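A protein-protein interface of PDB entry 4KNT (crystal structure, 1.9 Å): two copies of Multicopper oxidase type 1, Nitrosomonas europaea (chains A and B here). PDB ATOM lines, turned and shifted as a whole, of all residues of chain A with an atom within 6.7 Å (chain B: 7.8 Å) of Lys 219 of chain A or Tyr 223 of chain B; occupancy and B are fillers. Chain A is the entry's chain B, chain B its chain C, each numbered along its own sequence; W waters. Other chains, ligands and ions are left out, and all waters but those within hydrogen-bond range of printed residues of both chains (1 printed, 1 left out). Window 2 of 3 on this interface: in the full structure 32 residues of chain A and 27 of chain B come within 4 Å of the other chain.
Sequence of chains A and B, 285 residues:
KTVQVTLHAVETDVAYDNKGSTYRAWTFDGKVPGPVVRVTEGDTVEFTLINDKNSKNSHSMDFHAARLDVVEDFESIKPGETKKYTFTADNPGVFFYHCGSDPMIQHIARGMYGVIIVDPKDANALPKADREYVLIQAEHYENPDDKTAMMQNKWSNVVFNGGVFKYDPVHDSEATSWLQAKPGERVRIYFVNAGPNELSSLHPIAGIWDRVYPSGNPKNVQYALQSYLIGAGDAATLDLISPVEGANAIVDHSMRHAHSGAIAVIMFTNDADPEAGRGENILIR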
ATOM      1  N   ASN A  91     -38.918  22.882  -6.039  1.00  0.00           N
ATOM      2  CA  ASN A  91     -38.058  22.510  -7.153  1.00  0.00           C
ATOM      3  C   ASN A  91     -38.827  22.218  -8.440  1.00  0.00           C
ATOM      4  O   ASN A  91     -39.831  21.501  -8.413  1.00  0.00           O
ATOM      5  CB  ASN A  91     -37.193  21.304  -6.766  1.00  0.00           C
ATOM      6  CG  ASN A  91     -36.208  21.631  -5.662  1.00  0.00           C
ATOM      7  OD1 ASN A  91     -35.181  22.271  -5.898  1.00  0.00           O
ATOM      8  ND2 ASN A  91     -36.516  21.197  -4.452  1.00  0.00           N
ATOM      9  N   TYR A 213     -33.966  15.232 -18.897  1.00  0.00           N
ATOM     10  CA  TYR A 213     -33.806  15.944 -17.632  1.00  0.00           C
ATOM     11  C   TYR A 213     -34.169  15.047 -16.457  1.00  0.00           C
ATOM     12  O   TYR A 213     -35.351  14.815 -16.210  1.00  0.00           O
ATOM     13  CB  TYR A 213     -34.694  17.188 -17.595  1.00  0.00           C
ATOM     14  CG  TYR A 213     -34.451  18.180 -18.706  1.00  0.00           C
ATOM     15  CD1 TYR A 213     -33.538  19.217 -18.544  1.00  0.00           C
ATOM     16  CD2 TYR A 213     -35.151  18.097 -19.911  1.00  0.00           C
ATOM     17  CE1 TYR A 213     -33.314  20.141 -19.551  1.00  0.00           C
ATOM     18  CE2 TYR A 213     -34.932  19.022 -20.933  1.00  0.00           C
ATOM     19  CZ  TYR A 213     -34.012  20.037 -20.741  1.00  0.00           C
ATOM     20  OH  TYR A 213     -33.785  20.961 -21.731  1.00  0.00           O
ATOM     21  N   PRO A 214     -33.153  14.534 -15.733  1.00  0.00           N
ATOM     22  CA  PRO A 214     -33.369  13.807 -14.474  1.00  0.00           C
ATOM     23  C   PRO A 214     -34.223  14.602 -13.476  1.00  0.00           C
ATOM     24  O   PRO A 214     -33.888  15.743 -13.135  1.00  0.00           O
ATOM     25  CB  PRO A 214     -31.948  13.618 -13.942  1.00  0.00           C
ATOM     26  CG  PRO A 214     -31.114  13.521 -15.182  1.00  0.00           C
ATOM     27  CD  PRO A 214     -31.740  14.492 -16.152  1.00  0.00           C
ATOM     28  N   SER A 215     -35.324  13.987 -13.034  1.00  0.00           N
ATOM     29  CA  SER A 215     -36.337  14.635 -12.187  1.00  0.00           C
ATOM     30  C   SER A 215     -36.950  15.884 -12.831  1.00  0.00           C
ATOM     31  O   SER A 215     -37.581  16.691 -12.149  1.00  0.00           O
ATOM     32  CB  SER A 215     -35.789  14.948 -10.784  1.00  0.00           C
ATOM     33  OG  SER A 215     -35.782  13.784  -9.975  1.00  0.00           O
ATOM     34  N   GLY A 216     -36.761  16.028 -14.141  1.00  0.00           N
ATOM     35  CA  GLY A 216     -37.291  17.170 -14.889  1.00  0.00           C
ATOM     36  C   GLY A 216     -36.566  18.488 -14.667  1.00  0.00           C
ATOM     37  O   GLY A 216     -37.001  19.528 -15.171  1.00  0.00           O
ATOM     38  N   ASN A 217     -35.463  18.455 -13.922  1.00  0.00           N
ATOM     39  CA  ASN A 217     -34.751  19.684 -13.565  1.00  0.00           C
ATOM     40  C   ASN A 217     -33.816  20.151 -14.681  1.00  0.00           C
ATOM     41  O   ASN A 217     -32.959  19.387 -15.126  1.00  0.00           O
ATOM     42  CB  ASN A 217     -33.986  19.516 -12.244  1.00  0.00           C
ATOM     43  CG  ASN A 217     -33.664  20.849 -11.582  1.00  0.00           C
ATOM     44  OD1 ASN A 217     -32.910  21.663 -12.125  1.00  0.00           O
ATOM     45  ND2 ASN A 217     -34.243  21.080 -10.401  1.00  0.00           N
ATOM     46  N   PRO A 218     -33.983  21.409 -15.139  1.00  0.00           N
ATOM     47  CA  PRO A 218     -33.157  21.963 -16.222  1.00  0.00           C
ATOM     48  C   PRO A 218     -31.650  21.861 -15.971  1.00  0.00           C
ATOM     49  O   PRO A 218     -30.882  21.726 -16.923  1.00  0.00           O
ATOM     50  CB  PRO A 218     -33.591  23.432 -16.276  1.00  0.00           C
ATOM     51  CG  PRO A 218     -34.999  23.420 -15.778  1.00  0.00           C
ATOM     52  CD  PRO A 218     -35.022  22.362 -14.702  1.00  0.00           C
ATOM     53  N   LYS A 219     -31.239  21.902 -14.704  1.00  0.00           N
ATOM     54  CA  LYS A 219     -29.818  21.843 -14.331  1.00  0.00           C
ATOM     55  C   LYS A 219     -29.133  20.508 -14.636  1.00  0.00           C
ATOM     56  O   LYS A 219     -27.902  20.442 -14.692  1.00  0.00           O
ATOM     57  CB  LYS A 219     -29.637  22.154 -12.842  1.00  0.00           C
ATOM     58  CG  LYS A 219     -30.025  23.560 -12.405  1.00  0.00           C
ATOM     59  CD  LYS A 219     -29.618  23.757 -10.957  1.00  0.00           C
ATOM     60  CE  LYS A 219     -30.277  24.967 -10.333  1.00  0.00           C
ATOM     61  NZ  LYS A 219     -29.884  25.093  -8.895  1.00  0.00           N
ATOM     62  N   ASN A 220     -29.923  19.450 -14.822  1.00  0.00           N
ATOM     63  CA  ASN A 220     -29.385  18.095 -14.983  1.00  0.00           C
ATOM     64  C   ASN A 220     -29.371  17.591 -16.434  1.00  0.00           C
ATOM     65  O   ASN A 220     -29.204  16.397 -16.676  1.00  0.00           O
ATOM     66  CB  ASN A 220     -30.160  17.104 -14.097  1.00  0.00           C
ATOM     67  CG  ASN A 220     -30.121  17.473 -12.616  1.00  0.00           C
ATOM     68  OD1 ASN A 220     -29.110  17.954 -12.104  1.00  0.00           O
ATOM     69  ND2 ASN A 220     -31.227  17.234 -11.922  1.00  0.00           N
ATOM     70  N   VAL A 221     -29.527  18.502 -17.388  1.00  0.00           N
ATOM     71  CA  VAL A 221     -29.694  18.140 -18.805  1.00  0.00           C
ATOM     72  C   VAL A 221     -28.620  17.191 -19.373  1.00  0.00           C
ATOM     73  O   VAL A 221     -27.422  17.371 -19.143  1.00  0.00           O
ATOM     74  CB  VAL A 221     -29.861  19.409 -19.711  1.00  0.00           C
ATOM     75  CG1 VAL A 221     -28.612  20.284 -19.686  1.00  0.00           C
ATOM     76  CG2 VAL A 221     -30.235  19.024 -21.143  1.00  0.00           C
ATOM     77  N   ILE B 208     -36.253  15.414  -0.631  1.00  0.00           N
ATOM     78  CA  ILE B 208     -35.631  15.386  -1.950  1.00  0.00           C
ATOM     79  C   ILE B 208     -34.121  15.444  -1.752  1.00  0.00           C
ATOM     80  O   ILE B 208     -33.641  16.038  -0.785  1.00  0.00           O
ATOM     81  CB  ILE B 208     -36.136  16.561  -2.854  1.00  0.00           C
ATOM     82  CG1 ILE B 208     -35.752  16.341  -4.325  1.00  0.00           C
ATOM     83  CG2 ILE B 208     -35.645  17.931  -2.335  1.00  0.00           C
ATOM     84  CD1 ILE B 208     -36.496  17.241  -5.307  1.00  0.00           C
ATOM     85  N   TRP B 209     -33.371  14.813  -2.647  1.00  0.00           N
ATOM     86  CA  TRP B 209     -31.921  14.943  -2.618  1.00  0.00           C
ATOM     87  C   TRP B 209     -31.553  16.329  -3.132  1.00  0.00           C
ATOM     88  O   TRP B 209     -31.805  16.654  -4.297  1.00  0.00           O
ATOM     89  CB  TRP B 209     -31.239  13.855  -3.452  1.00  0.00           C
ATOM     90  CG  TRP B 209     -31.572  12.435  -3.044  1.00  0.00           C
ATOM     91  CD1 TRP B 209     -32.130  11.468  -3.834  1.00  0.00           C
ATOM     92  CD2 TRP B 209     -31.368  11.831  -1.756  1.00  0.00           C
ATOM     93  NE1 TRP B 209     -32.285  10.300  -3.120  1.00  0.00           N
ATOM     94  CE2 TRP B 209     -31.826  10.497  -1.842  1.00  0.00           C
ATOM     95  CE3 TRP B 209     -30.846  12.289  -0.536  1.00  0.00           C
ATOM     96  CZ2 TRP B 209     -31.780   9.614  -0.755  1.00  0.00           C
ATOM     97  CZ3 TRP B 209     -30.799  11.408   0.545  1.00  0.00           C
ATOM     98  CH2 TRP B 209     -31.263  10.088   0.426  1.00  0.00           C
ATOM     99  N   ASP B 210     -30.975  17.147  -2.257  1.00  0.00           N
ATOM    100  CA  ASP B 210     -30.493  18.475  -2.637  1.00  0.00           C
ATOM    101  C   ASP B 210     -29.477  18.382  -3.776  1.00  0.00           C
ATOM    102  O   ASP B 210     -29.555  19.115  -4.764  1.00  0.00           O
ATOM    103  CB  ASP B 210     -29.839  19.173  -1.441  1.00  0.00           C
ATOM    104  CG  ASP B 210     -29.400  20.585  -1.770  1.00  0.00           C
ATOM    105  OD1 ASP B 210     -30.276  21.474  -1.818  1.00  0.00           O
ATOM    106  OD2 ASP B 210     -28.188  20.801  -1.985  1.00  0.00           O
ATOM    107  N   ARG B 211     -28.519  17.475  -3.606  1.00  0.00           N
ATOM    108  CA  ARG B 211     -27.439  17.253  -4.551  1.00  0.00           C
ATOM    109  C   ARG B 211     -27.093  15.774  -4.521  1.00  0.00           C
ATOM    110  O   ARG B 211     -27.195  15.136  -3.475  1.00  0.00           O
ATOM    111  CB  ARG B 211     -26.200  18.054  -4.138  1.00  0.00           C
ATOM    112  CG  ARG B 211     -26.208  19.522  -4.526  1.00  0.00           C
ATOM    113  CD  ARG B 211     -25.161  20.281  -3.721  1.00  0.00           C
ATOM    114  NE  ARG B 211     -24.788  21.553  -4.343  1.00  0.00           N
ATOM    115  CZ  ARG B 211     -25.409  22.710  -4.130  1.00  0.00           C
ATOM    116  NH1 ARG B 211     -26.450  22.778  -3.309  1.00  0.00           N
ATOM    117  NH2 ARG B 211     -24.989  23.807  -4.748  1.00  0.00           N
ATOM    118  N   VAL B 212     -26.687  15.230  -5.663  1.00  0.00           N
ATOM    119  CA  VAL B 212     -26.161  13.865  -5.725  1.00  0.00           C
ATOM    120  C   VAL B 212     -24.847  13.859  -6.502  1.00  0.00           C
ATOM    121  O   VAL B 212     -24.729  14.520  -7.541  1.00  0.00           O
ATOM    122  CB  VAL B 212     -27.162  12.869  -6.373  1.00  0.00           C
ATOM    123  CG1 VAL B 212     -26.561  11.469  -6.451  1.00  0.00           C
ATOM    124  CG2 VAL B 212     -28.470  12.827  -5.590  1.00  0.00           C
ATOM    125  N   TYR B 213     -23.866  13.122  -5.985  1.00  0.00           N
ATOM    126  CA  TYR B 213     -22.558  13.003  -6.619  1.00  0.00           C
ATOM    127  C   TYR B 213     -22.251  11.542  -6.926  1.00  0.00           C
ATOM    128  O   TYR B 213     -21.917  10.788  -6.012  1.00  0.00           O
ATOM    129  CB  TYR B 213     -21.458  13.547  -5.703  1.00  0.00           C
ATOM    130  CG  TYR B 213     -21.634  14.978  -5.257  1.00  0.00           C
ATOM    131  CD1 TYR B 213     -21.094  16.022  -6.000  1.00  0.00           C
ATOM    132  CD2 TYR B 213     -22.314  15.286  -4.077  1.00  0.00           C
ATOM    133  CE1 TYR B 213     -21.231  17.340  -5.591  1.00  0.00           C
ATOM    134  CE2 TYR B 213     -22.460  16.608  -3.656  1.00  0.00           C
ATOM    135  CZ  TYR B 213     -21.916  17.627  -4.424  1.00  0.00           C
ATOM    136  OH  TYR B 213     -22.044  18.938  -4.032  1.00  0.00           O
ATOM    137  N   PRO B 218     -17.143  15.546  -6.928  1.00  0.00           N
ATOM    138  CA  PRO B 218     -17.722  16.882  -7.085  1.00  0.00           C
ATOM    139  C   PRO B 218     -18.022  17.276  -8.537  1.00  0.00           C
ATOM    140  O   PRO B 218     -18.957  18.033  -8.772  1.00  0.00           O
ATOM    141  CB  PRO B 218     -16.645  17.791  -6.491  1.00  0.00           C
ATOM    142  CG  PRO B 218     -16.018  16.942  -5.432  1.00  0.00           C
ATOM    143  CD  PRO B 218     -15.951  15.575  -6.058  1.00  0.00           C
ATOM    144  N   ASN B 220     -19.354  15.530 -10.865  1.00  0.00           N
ATOM    145  CA  ASN B 220     -20.514  14.834 -11.432  1.00  0.00           C
ATOM    146  C   ASN B 220     -21.860  15.282 -10.848  1.00  0.00           C
ATOM    147  O   ASN B 220     -22.882  14.622 -11.048  1.00  0.00           O
ATOM    148  CB  ASN B 220     -20.347  13.312 -11.276  1.00  0.00           C
ATOM    149  CG  ASN B 220     -19.089  12.783 -11.946  1.00  0.00           C
ATOM    150  OD1 ASN B 220     -18.697  13.245 -13.020  1.00  0.00           O
ATOM    151  ND2 ASN B 220     -18.454  11.798 -11.315  1.00  0.00           N
ATOM    152  N   VAL B 221     -21.856  16.417 -10.151  1.00  0.00           N
ATOM    153  CA  VAL B 221     -23.023  16.887  -9.390  1.00  0.00           C
ATOM    154  C   VAL B 221     -24.340  16.951 -10.183  1.00  0.00           C
ATOM    155  O   VAL B 221     -24.390  17.455 -11.307  1.00  0.00           O
ATOM    156  CB  VAL B 221     -22.736  18.252  -8.674  1.00  0.00           C
ATOM    157  CG1 VAL B 221     -22.475  19.372  -9.681  1.00  0.00           C
ATOM    158  CG2 VAL B 221     -23.867  18.624  -7.716  1.00  0.00           C
ATOM    159  N   GLN B 222     -25.385  16.387  -9.585  1.00  0.00           N
ATOM    160  CA  GLN B 222     -26.737  16.549 -10.099  1.00  0.00           C
ATOM    161  C   GLN B 222     -27.583  17.195  -9.012  1.00  0.00           C
ATOM    162  O   GLN B 222     -27.270  17.084  -7.825  1.00  0.00           O
ATOM    163  CB  GLN B 222     -27.331  15.212 -10.544  1.00  0.00           C
ATOM    164  CG  GLN B 222     -26.794  14.703 -11.882  1.00  0.00           C
ATOM    165  CD  GLN B 222     -27.450  13.403 -12.312  1.00  0.00           C
ATOM    166  OE1 GLN B 222     -28.658  13.350 -12.545  1.00  0.00           O
ATOM    167  NE2 GLN B 222     -26.653  12.347 -12.422  1.00  0.00           N
ATOM    168  N   TYR B 223     -28.640  17.893  -9.421  1.00  0.00           N
ATOM    169  CA  TYR B 223     -29.432  18.693  -8.482  1.00  0.00           C
ATOM    170  C   TYR B 223     -30.873  18.242  -8.316  1.00  0.00           C
ATOM    171  O   TYR B 223     -31.504  17.793  -9.272  1.00  0.00           O
ATOM    172  CB  TYR B 223     -29.414  20.168  -8.895  1.00  0.00           C
ATOM    173  CG  TYR B 223     -28.031  20.775  -8.933  1.00  0.00           C
ATOM    174  CD1 TYR B 223     -27.446  21.299  -7.779  1.00  0.00           C
ATOM    175  CD2 TYR B 223     -27.307  20.824 -10.123  1.00  0.00           C
ATOM    176  CE1 TYR B 223     -26.166  21.857  -7.812  1.00  0.00           C
ATOM    177  CE2 TYR B 223     -26.029  21.375 -10.166  1.00  0.00           C
ATOM    178  CZ  TYR B 223     -25.469  21.892  -9.010  1.00  0.00           C
ATOM    179  OH  TYR B 223     -24.208  22.440  -9.055  1.00  0.00           O
ATOM    180  N   ALA B 224     -31.380  18.391  -7.092  1.00  0.00           N
ATOM    181  CA  ALA B 224     -32.802  18.219  -6.781  1.00  0.00           C
ATOM    182  C   ALA B 224     -33.404  16.963  -7.404  1.00  0.00           C
ATOM    183  O   ALA B 224     -34.349  17.037  -8.201  1.00  0.00           O
ATOM    184  CB  ALA B 224     -33.599  19.479  -7.179  1.00  0.00           C
ATOM    185  N   LEU B 225     -32.841  15.812  -7.041  1.00  0.00           N
ATOM    186  CA  LEU B 225     -33.316  14.526  -7.548  1.00  0.00           C
ATOM    187  C   LEU B 225     -34.226  13.852  -6.531  1.00  0.00           C
ATOM    188  O   LEU B 225     -33.874  13.730  -5.359  1.00  0.00           O
ATOM    189  CB  LEU B 225     -32.140  13.598  -7.877  1.00  0.00           C
ATOM    190  CG  LEU B 225     -31.089  14.007  -8.916  1.00  0.00           C
ATOM    191  CD1 LEU B 225     -30.018  12.920  -9.005  1.00  0.00           C
ATOM    192  CD2 LEU B 225     -31.711  14.265 -10.287  1.00  0.00           C
ATOM    193  N   GLN B 226     -35.394  13.404  -6.982  1.00  0.00           N
ATOM    194  CA  GLN B 226     -36.303  12.686  -6.093  1.00  0.00           C
ATOM    195  C   GLN B 226     -35.760  11.298  -5.777  1.00  0.00           C
ATOM    196  O   GLN B 226     -35.967  10.775  -4.683  1.00  0.00           O
ATOM    197  CB  GLN B 226     -37.713  12.602  -6.683  1.00  0.00           C
ATOM    198  CG  GLN B 226     -37.832  11.782  -7.959  1.00  0.00           C
ATOM    199  CD  GLN B 226     -39.023  12.200  -8.781  1.00  0.00           C
ATOM    200  OE1 GLN B 226     -40.170  11.901  -8.440  1.00  0.00           O
ATOM    201  NE2 GLN B 226     -38.759  12.906  -9.874  1.00  0.00           N
HETATM  202  O   HOH W   1     -35.864  18.950  -9.491  1.00  0.00           O
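The side-chain hydroxyl (OG) of Ser 215 of chain A sits at hydrogen-bond distance from the backbone NH (N) of Gln 226 of chain B (3.0 Å).
The side-chain amide nitrogen (ND2) of Asn 220 of chain A lies within hydrogen-bond range of the backbone carbonyl oxygen (O) of Tyr 223 of chain B, 2.7 Å away.
N of Ala 224 of chain B sits at hydrogen-bond distance from O of Asp 210 of chain B (3.0 Å).
O of Trp 209 of chain B lies close to N of Ala 224 of chain B (3.3 Å).
The backbone NH of Lys 219 of chain A sits at hydrogen-bond distance from the side-chain amide oxygen of Asn 217 of chain A, at 3.1 Å.
The backbone carbonyl oxygen (O) of Leu 225 of chain B is in hydrogen-bond range of the backbone NH (N) of Trp 209 of chain B (3.0 Å).
O of Val 212 of chain B lies within hydrogen-bond range of N of Gln 222 of chain B, at 2.8 Å.
O of Pro 214 of chain A sits at hydrogen-bond distance from ND2 of Asn 220 of chain A, at 3.3 Å.
Asn 91 of chain A touches Ile 208 of chain B.
CB of Ala 224 of chain B touches OD1 of Asn 91 of chain A (3.5 Å).
OE1 of Gln 222 of chain B touches CB of Pro 214 of chain A, 3.6 Å away.
Pro 214 of chain A touches Leu 225 of chain B.
CB of Ser 215 of chain A touches O of Ala 224 of chain B, at 3.6 Å.
Leu 225 of chain B touches Ser 215 of chain A.
ND2 of Asn 217 of chain A touches CB of Ala 224 of chain B, at 3.7 Å.
CD2 of Tyr 223 of chain B touches CB of Lys 219 of chain A (3.8 Å).
CA of Gln 222 of chain B touches OD1 of Asn 220 of chain A (3.4 Å).
Asn 220 of chain A touches Leu 225 of chain B (ND2 to CD2, 3.4 Å).
Of chain B, only Tyr 223 (3.8 Å) comes within 4 Å of Lys 219 of chain A.
Of the printed residues of chain A, Gln 222 of chain B touches Pro 214 and Asn 220.
Of the printed residues of chain A, Leu 225 of chain B touches Pro 214, Ser 215 and Asn 220.
Of the printed residues of chain B, Asn 220 of chain A touches Gln 222 (3.4 Å), Tyr 223 (2.7 Å) and Leu 225 (3.4 Å).
Printed residues of chain A within 4 Å of Gln 226 of chain B: Ser 215.
Of the printed residues of chain B, Asn 217 of chain A touches Ala 224 (3.7 Å).
Asp 210 of chain B touches none of the printed residues of chain A.
The nearest residue of chain B that does not touch Lys 219 of chain A is Val 221 of chain B (5.7 Å).
The nearest printed residue of chain A that does not touch Leu 225 of chain B is Asn 217 of chain A (6.0 Å).
Of the 14 printed residues of chain B, 6 touch a printed residue of chain A.
Printed residues of chain B that touch a printed residue of chain A: Ile 208, Gln 222, Tyr 223, Ala 224, Leu 225 and Gln 226.
Hydrophobic or aromatic side chains of chain A that line the printed part of chain B: Pro 214.
Among the printed residues, 12 pairs touch across the chains.
Among the printed residues, no Asp or Glu carboxylate lies within 4 Å of a Lys or Arg side-chain nitrogen of the other chain.
Positions printed for both chains: 213, 218, 220 and 221.
Water W1 bridges the backbone carbonyl oxygen (O) of Ala 224 of chain B and the side-chain amide nitrogen (ND2) of Asn 217 of chain A.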
